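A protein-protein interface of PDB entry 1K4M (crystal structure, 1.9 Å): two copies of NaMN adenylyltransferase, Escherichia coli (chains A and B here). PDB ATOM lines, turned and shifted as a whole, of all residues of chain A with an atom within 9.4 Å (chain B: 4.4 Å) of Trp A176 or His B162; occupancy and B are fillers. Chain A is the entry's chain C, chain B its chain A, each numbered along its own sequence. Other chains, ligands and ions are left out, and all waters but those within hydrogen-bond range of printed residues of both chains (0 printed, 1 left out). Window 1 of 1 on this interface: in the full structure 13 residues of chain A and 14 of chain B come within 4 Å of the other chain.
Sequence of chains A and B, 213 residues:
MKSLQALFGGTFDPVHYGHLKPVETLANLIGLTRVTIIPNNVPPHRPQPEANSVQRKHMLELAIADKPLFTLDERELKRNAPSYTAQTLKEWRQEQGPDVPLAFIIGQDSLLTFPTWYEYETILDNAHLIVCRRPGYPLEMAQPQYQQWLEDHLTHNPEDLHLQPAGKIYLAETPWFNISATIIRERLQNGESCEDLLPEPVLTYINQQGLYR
The backbone carbonyl oxygen (O) of Ile B30 is in hydrogen-bond range of the backbone NH (N) of Trp A176, 3.1 Å away. OE2 of Glu B159 sits at hydrogen-bond distance from N of Gly A136 (2.8 Å). O of His B162 lies within hydrogen-bond range of ND2 of Asn A178 (2.9 Å).
The backbone carbonyl oxygen of Ile B30 is in hydrogen-bond range of a ring nitrogen (NE2) of His B162, 2.8 Å away. The side-chain amide oxygen of Asn B157 is in hydrogen-bond range of the backbone NH of Glu B159 (2.9 Å).
Among the printed residues, pairs that only touch across the chains: Pro A135 with Glu B159 (3.2 Å), Gly A136 with Leu B163 (3.8 Å), Pro A175 with Ile B30 (3.8 Å), Pro A175 with Gly B31 (3.5 Å), Trp A176 with Gly B31 (3.5 Å), Trp A176 with Pro B158 (3.4 Å), Trp A176 with Glu B159 (3.7 Å), Trp A176 with His B162 (3.0 Å), Phe A177 with Gly B31 (3.6 Å) and Asn A178 with Met B1 (3.7 Å).
Printed residues of chain B within 4 Å of Pro A135: Glu B159. Of the printed residues of chain B, Pro A175 touches Ile B30 and Gly B31. Of the printed residues of chain B, Trp A176 touches Ile B30, Gly B31, Pro B158, Glu B159 and His B162. Of the printed residues of chain B, Phe A177 touches Gly B31 (3.6 Å). Printed residues of chain B within 4 Å of Asn A178: Met B1 and His B162. Of chain A, only Pro A175 (3.5 Å), Trp A176 (3.5 Å) and Phe A177 (3.6 Å) come within 4 Å of Gly B31. Glu B159 touches just these residues of chain A: Pro A135 (3.2 Å), Gly A136 (2.8 Å) and Trp A176 (3.7 Å). Of chain A, only Trp A176 and Asn A178 come within 4 Å of His B162. Leu B163 touches one residue of chain A.
Hydrophobic or aromatic side chains of chain A within 4 Å of the printed part of chain B: Pro A175, Trp A176 and Phe A177. Hydrophobic or aromatic side chains of chain B that line the printed part of chain A: Met B1, Pro B158, His B162 and Leu B163. Among the printed residues, no Asp or Glu carboxylate lies within 4 Å of a Lys or Arg side-chain nitrogen of the other chain.
No position is printed for both chains. Of the 13 pairs that touch across the chains among the printed residues, none has its exchanged pair printed and touching as well.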
ATOM      1  N   TYR A  17     -16.619 -12.859 -19.847  1.00  0.00           N
ATOM      2  CA  TYR A  17     -17.751 -13.645 -20.349  1.00  0.00           C
ATOM      3  C   TYR A  17     -18.017 -14.932 -19.580  1.00  0.00           C
ATOM      4  O   TYR A  17     -19.136 -15.442 -19.594  1.00  0.00           O
ATOM      5  CB  TYR A  17     -17.544 -13.963 -21.831  1.00  0.00           C
ATOM      6  CG  TYR A  17     -17.723 -12.758 -22.729  1.00  0.00           C
ATOM      7  CD1 TYR A  17     -16.937 -12.594 -23.868  1.00  0.00           C
ATOM      8  CD2 TYR A  17     -18.681 -11.781 -22.434  1.00  0.00           C
ATOM      9  CE1 TYR A  17     -17.091 -11.494 -24.698  1.00  0.00           C
ATOM     10  CE2 TYR A  17     -18.851 -10.665 -23.256  1.00  0.00           C
ATOM     11  CZ  TYR A  17     -18.053 -10.533 -24.394  1.00  0.00           C
ATOM     12  OH  TYR A  17     -18.262  -9.472 -25.255  1.00  0.00           O
ATOM     13  N   GLY A  18     -16.987 -15.468 -18.936  1.00  0.00           N
ATOM     14  CA  GLY A  18     -17.148 -16.681 -18.148  1.00  0.00           C
ATOM     15  C   GLY A  18     -18.025 -16.408 -16.935  1.00  0.00           C
ATOM     16  O   GLY A  18     -18.643 -17.330 -16.382  1.00  0.00           O
ATOM     17  N   HIS A  19     -18.066 -15.143 -16.511  1.00  0.00           N
ATOM     18  CA  HIS A  19     -18.883 -14.728 -15.374  1.00  0.00           C
ATOM     19  C   HIS A  19     -20.296 -14.439 -15.855  1.00  0.00           C
ATOM     20  O   HIS A  19     -21.297 -14.866 -15.264  1.00  0.00           O
ATOM     21  CB  HIS A  19     -18.409 -13.398 -14.756  1.00  0.00           C
ATOM     22  CG  HIS A  19     -17.021 -13.416 -14.174  1.00  0.00           C
ATOM     23  ND1 HIS A  19     -16.623 -14.299 -13.190  1.00  0.00           N
ATOM     24  CD2 HIS A  19     -15.945 -12.634 -14.431  1.00  0.00           C
ATOM     25  CE1 HIS A  19     -15.360 -14.067 -12.876  1.00  0.00           C
ATOM     26  NE2 HIS A  19     -14.924 -13.062 -13.615  1.00  0.00           N
ATOM     27  N   LYS A  21     -21.962 -14.819 -19.221  1.00  0.00           N
ATOM     28  CA  LYS A  21     -22.780 -15.646 -20.088  1.00  0.00           C
ATOM     29  C   LYS A  21     -23.490 -16.806 -19.425  1.00  0.00           C
ATOM     30  O   LYS A  21     -24.626 -17.074 -19.749  1.00  0.00           O
ATOM     31  CB  LYS A  21     -21.976 -16.090 -21.298  1.00  0.00           C
ATOM     32  CG  LYS A  21     -21.504 -14.908 -22.154  1.00  0.00           C
ATOM     33  CD  LYS A  21     -20.957 -15.422 -23.500  1.00  0.00           C
ATOM     34  CE  LYS A  21     -20.533 -14.277 -24.403  1.00  0.00           C
ATOM     35  NZ  LYS A  21     -21.693 -13.437 -24.800  1.00  0.00           N
ATOM     36  N   PRO A  22     -22.829 -17.515 -18.484  1.00  0.00           N
ATOM     37  CA  PRO A  22     -23.553 -18.621 -17.851  1.00  0.00           C
ATOM     38  C   PRO A  22     -24.784 -18.072 -17.143  1.00  0.00           C
ATOM     39  O   PRO A  22     -25.873 -18.639 -17.229  1.00  0.00           O
ATOM     40  CB  PRO A  22     -22.540 -19.184 -16.849  1.00  0.00           C
ATOM     41  CG  PRO A  22     -21.242 -18.981 -17.569  1.00  0.00           C
ATOM     42  CD  PRO A  22     -21.404 -17.538 -18.101  1.00  0.00           C
ATOM     43  N   VAL A  23     -24.616 -16.943 -16.473  1.00  0.00           N
ATOM     44  CA  VAL A  23     -25.728 -16.359 -15.728  1.00  0.00           C
ATOM     45  C   VAL A  23     -26.852 -15.834 -16.613  1.00  0.00           C
ATOM     46  O   VAL A  23     -28.039 -15.968 -16.276  1.00  0.00           O
ATOM     47  CB  VAL A  23     -25.232 -15.232 -14.771  1.00  0.00           C
ATOM     48  CG1 VAL A  23     -26.428 -14.559 -14.079  1.00  0.00           C
ATOM     49  CG2 VAL A  23     -24.279 -15.821 -13.735  1.00  0.00           C
ATOM     50  N   THR A  25     -27.790 -16.990 -19.489  1.00  0.00           N
ATOM     51  CA  THR A  25     -28.531 -18.158 -19.962  1.00  0.00           C
ATOM     52  C   THR A  25     -29.340 -18.767 -18.820  1.00  0.00           C
ATOM     53  O   THR A  25     -30.397 -19.352 -19.041  1.00  0.00           O
ATOM     54  CB  THR A  25     -27.576 -19.219 -20.532  1.00  0.00           C
ATOM     55  OG1 THR A  25     -26.959 -18.700 -21.714  1.00  0.00           O
ATOM     56  CG2 THR A  25     -28.321 -20.496 -20.902  1.00  0.00           C
ATOM     57  N   GLN A 108     -19.105 -24.073 -10.594  1.00  0.00           N
ATOM     58  CA  GLN A 108     -18.706 -25.355 -10.026  1.00  0.00           C
ATOM     59  C   GLN A 108     -17.420 -25.263  -9.167  1.00  0.00           C
ATOM     60  O   GLN A 108     -17.325 -25.909  -8.134  1.00  0.00           O
ATOM     61  CB  GLN A 108     -18.504 -26.387 -11.139  1.00  0.00           C
ATOM     62  CG  GLN A 108     -18.130 -27.809 -10.657  1.00  0.00           C
ATOM     63  CD  GLN A 108     -19.230 -28.460  -9.822  1.00  0.00           C
ATOM     64  OE1 GLN A 108     -20.394 -28.050  -9.884  1.00  0.00           O
ATOM     65  NE2 GLN A 108     -18.870 -29.493  -9.044  1.00  0.00           N
ATOM     66  N   CYS A 132     -23.354 -23.013 -11.646  1.00  0.00           N
ATOM     67  CA  CYS A 132     -23.115 -22.995 -13.094  1.00  0.00           C
ATOM     68  C   CYS A 132     -21.942 -23.898 -13.438  1.00  0.00           C
ATOM     69  O   CYS A 132     -20.939 -23.920 -12.735  1.00  0.00           O
ATOM     70  CB  CYS A 132     -22.805 -21.576 -13.578  1.00  0.00           C
ATOM     71  SG  CYS A 132     -24.164 -20.441 -13.408  1.00  0.00           S
ATOM     72  N   ARG A 133     -22.056 -24.632 -14.529  1.00  0.00           N
ATOM     73  CA  ARG A 133     -21.001 -25.560 -14.932  1.00  0.00           C
ATOM     74  C   ARG A 133     -19.696 -24.869 -15.300  1.00  0.00           C
ATOM     75  O   ARG A 133     -19.687 -23.746 -15.769  1.00  0.00           O
ATOM     76  CB  ARG A 133     -21.459 -26.378 -16.130  1.00  0.00           C
ATOM     77  CG  ARG A 133     -22.799 -27.081 -15.931  1.00  0.00           C
ATOM     78  CD  ARG A 133     -23.093 -28.057 -17.063  1.00  0.00           C
ATOM     79  NE  ARG A 133     -23.591 -27.382 -18.252  1.00  0.00           N
ATOM     80  CZ  ARG A 133     -24.326 -27.990 -19.177  1.00  0.00           C
ATOM     81  NH1 ARG A 133     -24.623 -29.272 -19.044  1.00  0.00           N
ATOM     82  NH2 ARG A 133     -24.807 -27.308 -20.201  1.00  0.00           N
ATOM     83  N   ARG A 134     -18.586 -25.557 -15.079  1.00  0.00           N
ATOM     84  CA  ARG A 134     -17.304 -25.016 -15.462  1.00  0.00           C
ATOM     85  C   ARG A 134     -16.541 -26.231 -15.970  1.00  0.00           C
ATOM     86  O   ARG A 134     -16.371 -27.228 -15.262  1.00  0.00           O
ATOM     87  CB  ARG A 134     -16.633 -24.344 -14.266  1.00  0.00           C
ATOM     88  CG  ARG A 134     -15.526 -23.405 -14.696  1.00  0.00           C
ATOM     89  CD  ARG A 134     -15.118 -22.413 -13.610  1.00  0.00           C
ATOM     90  NE  ARG A 134     -13.995 -21.638 -14.120  1.00  0.00           N
ATOM     91  CZ  ARG A 134     -13.238 -20.828 -13.397  1.00  0.00           C
ATOM     92  NH1 ARG A 134     -13.477 -20.663 -12.110  1.00  0.00           N
ATOM     93  NH2 ARG A 134     -12.221 -20.199 -13.968  1.00  0.00           N
ATOM     94  N   PRO A 135     -16.080 -26.176 -17.226  1.00  0.00           N
ATOM     95  CA  PRO A 135     -15.356 -27.314 -17.799  1.00  0.00           C
ATOM     96  C   PRO A 135     -14.125 -27.783 -17.030  1.00  0.00           C
ATOM     97  O   PRO A 135     -13.384 -26.982 -16.470  1.00  0.00           O
ATOM     98  CB  PRO A 135     -15.027 -26.833 -19.217  1.00  0.00           C
ATOM     99  CG  PRO A 135     -14.918 -25.361 -19.066  1.00  0.00           C
ATOM    100  CD  PRO A 135     -16.029 -25.002 -18.119  1.00  0.00           C
ATOM    101  N   GLY A 136     -13.927 -29.092 -16.993  1.00  0.00           N
ATOM    102  CA  GLY A 136     -12.760 -29.626 -16.316  1.00  0.00           C
ATOM    103  C   GLY A 136     -12.818 -29.844 -14.813  1.00  0.00           C
ATOM    104  O   GLY A 136     -11.977 -30.560 -14.282  1.00  0.00           O
ATOM    105  N   TYR A 137     -13.788 -29.257 -14.117  1.00  0.00           N
ATOM    106  CA  TYR A 137     -13.853 -29.430 -12.665  1.00  0.00           C
ATOM    107  C   TYR A 137     -14.521 -30.690 -12.178  1.00  0.00           C
ATOM    108  O   TYR A 137     -15.392 -31.247 -12.840  1.00  0.00           O
ATOM    109  CB  TYR A 137     -14.536 -28.232 -11.999  1.00  0.00           C
ATOM    110  CG  TYR A 137     -13.696 -26.988 -12.085  1.00  0.00           C
ATOM    111  CD1 TYR A 137     -13.547 -26.319 -13.294  1.00  0.00           C
ATOM    112  CD2 TYR A 137     -12.989 -26.522 -10.979  1.00  0.00           C
ATOM    113  CE1 TYR A 137     -12.720 -25.214 -13.406  1.00  0.00           C
ATOM    114  CE2 TYR A 137     -12.151 -25.419 -11.083  1.00  0.00           C
ATOM    115  CZ  TYR A 137     -12.026 -24.769 -12.306  1.00  0.00           C
ATOM    116  OH  TYR A 137     -11.217 -23.667 -12.426  1.00  0.00           O
ATOM    117  N   LEU A 139     -17.054 -32.993 -10.319  1.00  0.00           N
ATOM    118  CA  LEU A 139     -18.466 -32.772 -10.066  1.00  0.00           C
ATOM    119  C   LEU A 139     -18.827 -33.148  -8.638  1.00  0.00           C
ATOM    120  O   LEU A 139     -19.864 -32.721  -8.117  1.00  0.00           O
ATOM    121  CB  LEU A 139     -19.322 -33.596 -11.031  1.00  0.00           C
ATOM    122  CG  LEU A 139     -19.244 -33.239 -12.514  1.00  0.00           C
ATOM    123  CD1 LEU A 139     -20.296 -34.062 -13.239  1.00  0.00           C
ATOM    124  CD2 LEU A 139     -19.498 -31.740 -12.732  1.00  0.00           C
ATOM    125  N   ALA A 172     -27.223 -26.182 -12.564  1.00  0.00           N
ATOM    126  CA  ALA A 172     -27.810 -25.748 -13.827  1.00  0.00           C
ATOM    127  C   ALA A 172     -26.999 -26.208 -15.040  1.00  0.00           C
ATOM    128  O   ALA A 172     -25.792 -26.397 -14.935  1.00  0.00           O
ATOM    129  CB  ALA A 172     -27.942 -24.248 -13.829  1.00  0.00           C
ATOM    130  N   GLU A 173     -27.681 -26.409 -16.167  1.00  0.00           N
ATOM    131  CA  GLU A 173     -27.047 -26.851 -17.401  1.00  0.00           C
ATOM    132  C   GLU A 173     -26.709 -25.639 -18.249  1.00  0.00           C
ATOM    133  O   GLU A 173     -27.302 -25.387 -19.307  1.00  0.00           O
ATOM    134  CB  GLU A 173     -27.978 -27.815 -18.148  1.00  0.00           C
ATOM    135  CG  GLU A 173     -28.350 -29.010 -17.270  1.00  0.00           C
ATOM    136  CD  GLU A 173     -28.903 -30.197 -18.035  1.00  0.00           C
ATOM    137  OE1 GLU A 173     -29.866 -30.029 -18.816  1.00  0.00           O
ATOM    138  OE2 GLU A 173     -28.367 -31.312 -17.835  1.00  0.00           O
ATOM    139  N   THR A 174     -25.728 -24.896 -17.766  1.00  0.00           N
ATOM    140  CA  THR A 174     -25.268 -23.674 -18.397  1.00  0.00           C
ATOM    141  C   THR A 174     -24.081 -23.857 -19.345  1.00  0.00           C
ATOM    142  O   THR A 174     -23.340 -24.830 -19.275  1.00  0.00           O
ATOM    143  CB  THR A 174     -24.898 -22.652 -17.309  1.00  0.00           C
ATOM    144  OG1 THR A 174     -24.053 -23.276 -16.323  1.00  0.00           O
ATOM    145  CG2 THR A 174     -26.170 -22.118 -16.632  1.00  0.00           C
ATOM    146  N   PRO A 175     -23.901 -22.908 -20.270  1.00  0.00           N
ATOM    147  CA  PRO A 175     -22.791 -22.981 -21.226  1.00  0.00           C
ATOM    148  C   PRO A 175     -21.418 -22.968 -20.542  1.00  0.00           C
ATOM    149  O   PRO A 175     -21.239 -22.349 -19.478  1.00  0.00           O
ATOM    150  CB  PRO A 175     -23.014 -21.765 -22.110  1.00  0.00           C
ATOM    151  CG  PRO A 175     -23.792 -20.791 -21.207  1.00  0.00           C
ATOM    152  CD  PRO A 175     -24.769 -21.746 -20.529  1.00  0.00           C
ATOM    153  N   TRP A 176     -20.470 -23.674 -21.152  1.00  0.00           N
ATOM    154  CA  TRP A 176     -19.093 -23.781 -20.648  1.00  0.00           C
ATOM    155  C   TRP A 176     -18.156 -22.740 -21.235  1.00  0.00           C
ATOM    156  O   TRP A 176     -18.270 -22.396 -22.414  1.00  0.00           O
ATOM    157  CB  TRP A 176     -18.494 -25.133 -21.010  1.00  0.00           C
ATOM    158  CG  TRP A 176     -19.107 -26.278 -20.338  1.00  0.00           C
ATOM    159  CD1 TRP A 176     -18.800 -26.762 -19.106  1.00  0.00           C
ATOM    160  CD2 TRP A 176     -20.114 -27.129 -20.872  1.00  0.00           C
ATOM    161  NE1 TRP A 176     -19.550 -27.871 -18.837  1.00  0.00           N
ATOM    162  CE2 TRP A 176     -20.369 -28.122 -19.907  1.00  0.00           C
ATOM    163  CE3 TRP A 176     -20.826 -27.150 -22.077  1.00  0.00           C
ATOM    164  CZ2 TRP A 176     -21.308 -29.134 -20.102  1.00  0.00           C
ATOM    165  CZ3 TRP A 176     -21.767 -28.160 -22.277  1.00  0.00           C
ATOM    166  CH2 TRP A 176     -21.997 -29.139 -21.292  1.00  0.00           C
ATOM    167  N   PHE A 177     -17.188 -22.279 -20.441  1.00  0.00           N
ATOM    168  CA  PHE A 177     -16.236 -21.311 -20.966  1.00  0.00           C
ATOM    169  C   PHE A 177     -14.862 -21.477 -20.346  1.00  0.00           C
ATOM    170  O   PHE A 177     -14.718 -21.403 -19.113  1.00  0.00           O
ATOM    171  CB  PHE A 177     -16.700 -19.881 -20.716  1.00  0.00           C
ATOM    172  CG  PHE A 177     -17.980 -19.530 -21.402  1.00  0.00           C
ATOM    173  CD1 PHE A 177     -19.202 -19.713 -20.755  1.00  0.00           C
ATOM    174  CD2 PHE A 177     -17.974 -18.987 -22.691  1.00  0.00           C
ATOM    175  CE1 PHE A 177     -20.403 -19.356 -21.372  1.00  0.00           C
ATOM    176  CE2 PHE A 177     -19.179 -18.625 -23.325  1.00  0.00           C
ATOM    177  CZ  PHE A 177     -20.394 -18.808 -22.664  1.00  0.00           C
ATOM    178  N   ASN A 178     -13.872 -21.726 -21.203  1.00  0.00           N
ATOM    179  CA  ASN A 178     -12.479 -21.867 -20.795  1.00  0.00           C
ATOM    180  C   ASN A 178     -11.934 -20.455 -20.668  1.00  0.00           C
ATOM    181  O   ASN A 178     -11.088 -20.028 -21.467  1.00  0.00           O
ATOM    182  CB  ASN A 178     -11.651 -22.578 -21.864  1.00  0.00           C
ATOM    183  CG  ASN A 178     -11.879 -24.063 -21.889  1.00  0.00           C
ATOM    184  OD1 ASN A 178     -12.328 -24.660 -20.900  1.00  0.00           O
ATOM    185  ND2 ASN A 178     -11.535 -24.690 -23.023  1.00  0.00           N
ATOM    186  N   ILE A 179     -12.426 -19.732 -19.672  1.00  0.00           N
ATOM    187  CA  ILE A 179     -12.005 -18.359 -19.442  1.00  0.00           C
ATOM    188  C   ILE A 179     -11.788 -18.106 -17.941  1.00  0.00           C
ATOM    189  O   ILE A 179     -12.549 -18.578 -17.102  1.00  0.00           O
ATOM    190  CB  ILE A 179     -13.074 -17.370 -19.946  1.00  0.00           C
ATOM    191  CG1 ILE A 179     -13.345 -17.627 -21.436  1.00  0.00           C
ATOM    192  CG2 ILE A 179     -12.621 -15.935 -19.707  1.00  0.00           C
ATOM    193  CD1 ILE A 179     -14.421 -16.749 -22.038  1.00  0.00           C
ATOM    194  N   MET B   1      -5.891 -25.898 -22.375  1.00  0.00           N
ATOM    195  CA  MET B   1      -7.016 -25.687 -23.342  1.00  0.00           C
ATOM    196  C   MET B   1      -7.550 -24.244 -23.337  1.00  0.00           C
ATOM    197  O   MET B   1      -8.012 -23.756 -22.325  1.00  0.00           O
ATOM    198  CB  MET B   1      -8.146 -26.662 -23.022  1.00  0.00           C
ATOM    199  CG  MET B   1      -8.820 -27.268 -24.235  1.00  0.00           C
ATOM    200  SD  MET B   1      -7.709 -28.212 -25.321  1.00  0.00           S
ATOM    201  CE  MET B   1      -7.702 -27.212 -26.723  1.00  0.00           C
ATOM    202  N   LEU B   4     -13.014 -22.203 -26.518  1.00  0.00           N
ATOM    203  CA  LEU B   4     -13.561 -22.851 -27.718  1.00  0.00           C
ATOM    204  C   LEU B   4     -14.004 -21.842 -28.799  1.00  0.00           C
ATOM    205  O   LEU B   4     -14.845 -20.970 -28.539  1.00  0.00           O
ATOM    206  CB  LEU B   4     -14.751 -23.734 -27.357  1.00  0.00           C
ATOM    207  CG  LEU B   4     -15.609 -24.181 -28.552  1.00  0.00           C
ATOM    208  CD1 LEU B   4     -14.837 -25.173 -29.441  1.00  0.00           C
ATOM    209  CD2 LEU B   4     -16.881 -24.822 -28.032  1.00  0.00           C
ATOM    210  N   ILE B  30     -23.874 -24.384 -25.680  1.00  0.00           N
ATOM    211  CA  ILE B  30     -22.575 -24.916 -25.341  1.00  0.00           C
ATOM    212  C   ILE B  30     -21.501 -23.940 -24.875  1.00  0.00           C
ATOM    213  O   ILE B  30     -20.578 -24.341 -24.168  1.00  0.00           O
ATOM    214  CB  ILE B  30     -22.052 -25.802 -26.470  1.00  0.00           C
ATOM    215  CG1 ILE B  30     -21.892 -25.013 -27.742  1.00  0.00           C
ATOM    216  CG2 ILE B  30     -23.056 -26.953 -26.729  1.00  0.00           C
ATOM    217  CD1 ILE B  30     -20.918 -25.656 -28.676  1.00  0.00           C
ATOM    218  N   GLY B  31     -21.629 -22.664 -25.242  1.00  0.00           N
ATOM    219  CA  GLY B  31     -20.667 -21.669 -24.805  1.00  0.00           C
ATOM    220  C   GLY B  31     -19.695 -21.247 -25.886  1.00  0.00           C
ATOM    221  O   GLY B  31     -18.563 -21.756 -25.971  1.00  0.00           O
ATOM    222  N   PRO B 101      -9.463 -25.159 -28.701  1.00  0.00           N
ATOM    223  CA  PRO B 101     -10.489 -26.087 -29.180  1.00  0.00           C
ATOM    224  C   PRO B 101     -11.138 -25.393 -30.352  1.00  0.00           C
ATOM    225  O   PRO B 101     -11.456 -24.209 -30.276  1.00  0.00           O
ATOM    226  CB  PRO B 101     -11.446 -26.222 -27.995  1.00  0.00           C
ATOM    227  CG  PRO B 101     -10.601 -25.771 -26.786  1.00  0.00           C
ATOM    228  CD  PRO B 101      -9.814 -24.624 -27.380  1.00  0.00           C
ATOM    229  N   ASN B 157     -21.516 -35.685 -24.559  1.00  0.00           N
ATOM    230  CA  ASN B 157     -21.174 -34.658 -23.565  1.00  0.00           C
ATOM    231  C   ASN B 157     -20.499 -33.471 -24.218  1.00  0.00           C
ATOM    232  O   ASN B 157     -19.295 -33.495 -24.465  1.00  0.00           O
ATOM    233  CB  ASN B 157     -20.236 -35.174 -22.462  1.00  0.00           C
ATOM    234  CG  ASN B 157     -20.073 -34.152 -21.324  1.00  0.00           C
ATOM    235  OD1 ASN B 157     -20.570 -33.003 -21.417  1.00  0.00           O
ATOM    236  ND2 ASN B 157     -19.385 -34.556 -20.246  1.00  0.00           N
ATOM    237  N   PRO B 158     -21.263 -32.410 -24.497  1.00  0.00           N
ATOM    238  CA  PRO B 158     -20.610 -31.267 -25.134  1.00  0.00           C
ATOM    239  C   PRO B 158     -19.445 -30.662 -24.362  1.00  0.00           C
ATOM    240  O   PRO B 158     -18.711 -29.826 -24.893  1.00  0.00           O
ATOM    241  CB  PRO B 158     -21.761 -30.294 -25.380  1.00  0.00           C
ATOM    242  CG  PRO B 158     -22.778 -30.665 -24.354  1.00  0.00           C
ATOM    243  CD  PRO B 158     -22.709 -32.178 -24.351  1.00  0.00           C
ATOM    244  N   GLU B 159     -19.258 -31.072 -23.112  1.00  0.00           N
ATOM    245  CA  GLU B 159     -18.129 -30.540 -22.349  1.00  0.00           C
ATOM    246  C   GLU B 159     -16.829 -30.969 -23.043  1.00  0.00           C
ATOM    247  O   GLU B 159     -15.832 -30.234 -23.032  1.00  0.00           O
ATOM    248  CB  GLU B 159     -18.132 -31.069 -20.914  1.00  0.00           C
ATOM    249  CG  GLU B 159     -17.089 -30.364 -20.033  1.00  0.00           C
ATOM    250  CD  GLU B 159     -16.997 -30.964 -18.644  1.00  0.00           C
ATOM    251  OE1 GLU B 159     -17.713 -31.963 -18.393  1.00  0.00           O
ATOM    252  OE2 GLU B 159     -16.202 -30.450 -17.812  1.00  0.00           O
ATOM    253  N   ASP B 160     -16.852 -32.163 -23.642  1.00  0.00           N
ATOM    254  CA  ASP B 160     -15.701 -32.708 -24.370  1.00  0.00           C
ATOM    255  C   ASP B 160     -15.189 -31.716 -25.417  1.00  0.00           C
ATOM    256  O   ASP B 160     -13.994 -31.705 -25.746  1.00  0.00           O
ATOM    257  CB  ASP B 160     -16.079 -33.994 -25.117  1.00  0.00           C
ATOM    258  CG  ASP B 160     -16.405 -35.157 -24.197  1.00  0.00           C
ATOM    259  OD1 ASP B 160     -16.996 -36.135 -24.680  1.00  0.00           O
ATOM    260  OD2 ASP B 160     -16.078 -35.108 -23.004  1.00  0.00           O
ATOM    261  N   LEU B 161     -16.089 -30.896 -25.958  1.00  0.00           N
ATOM    262  CA  LEU B 161     -15.699 -29.940 -26.993  1.00  0.00           C
ATOM    263  C   LEU B 161     -14.751 -28.879 -26.464  1.00  0.00           C
ATOM    264  O   LEU B 161     -13.948 -28.309 -27.219  1.00  0.00           O
ATOM    265  CB  LEU B 161     -16.935 -29.268 -27.583  1.00  0.00           C
ATOM    266  CG  LEU B 161     -17.990 -30.166 -28.212  1.00  0.00           C
ATOM    267  CD1 LEU B 161     -19.298 -29.376 -28.400  1.00  0.00           C
ATOM    268  CD2 LEU B 161     -17.465 -30.695 -29.545  1.00  0.00           C
ATOM    269  N   HIS B 162     -14.846 -28.616 -25.161  1.00  0.00           N
ATOM    270  CA  HIS B 162     -14.015 -27.622 -24.496  1.00  0.00           C
ATOM    271  C   HIS B 162     -12.767 -28.236 -23.908  1.00  0.00           C
ATOM    272  O   HIS B 162     -11.832 -27.527 -23.609  1.00  0.00           O
ATOM    273  CB  HIS B 162     -14.787 -26.936 -23.352  1.00  0.00           C
ATOM    274  CG  HIS B 162     -15.970 -26.136 -23.807  1.00  0.00           C
ATOM    275  ND1 HIS B 162     -15.912 -24.779 -24.040  1.00  0.00           N
ATOM    276  CD2 HIS B 162     -17.251 -26.507 -24.054  1.00  0.00           C
ATOM    277  CE1 HIS B 162     -17.110 -24.345 -24.406  1.00  0.00           C
ATOM    278  NE2 HIS B 162     -17.939 -25.375 -24.420  1.00  0.00           N
ATOM    279  N   LEU B 163     -12.757 -29.553 -23.735  1.00  0.00           N
ATOM    280  CA  LEU B 163     -11.604 -30.220 -23.143  1.00  0.00           C
ATOM    281  C   LEU B 163     -10.553 -30.829 -24.088  1.00  0.00           C
ATOM    282  O   LEU B 163      -9.510 -31.301 -23.610  1.00  0.00           O
ATOM    283  CB  LEU B 163     -12.092 -31.302 -22.186  1.00  0.00           C
ATOM    284  CG  LEU B 163     -12.906 -30.774 -21.002  1.00  0.00           C
ATOM    285  CD1 LEU B 163     -13.304 -31.953 -20.140  1.00  0.00           C
ATOM    286  CD2 LEU B 163     -12.108 -29.758 -20.213  1.00  0.00           C
ATOM    287  N   GLN B 164     -10.831 -30.854 -25.394  1.00  0.00           N
ATOM    288  CA  GLN B 164      -9.903 -31.395 -26.405  1.00  0.00           C
ATOM    289  C   GLN B 164      -9.897 -30.369 -27.507  1.00  0.00           C
ATOM    290  O   GLN B 164     -10.869 -29.641 -27.677  1.00  0.00           O
ATOM    291  CB  GLN B 164     -10.406 -32.690 -27.050  1.00  0.00           C
ATOM    292  CG  GLN B 164     -10.588 -33.861 -26.146  1.00  0.00           C
ATOM    293  CD  GLN B 164     -11.209 -35.029 -26.881  1.00  0.00           C
ATOM    294  OE1 GLN B 164     -11.221 -35.080 -28.128  1.00  0.00           O
ATOM    295  NE2 GLN B 164     -11.717 -35.985 -26.124  1.00  0.00           N
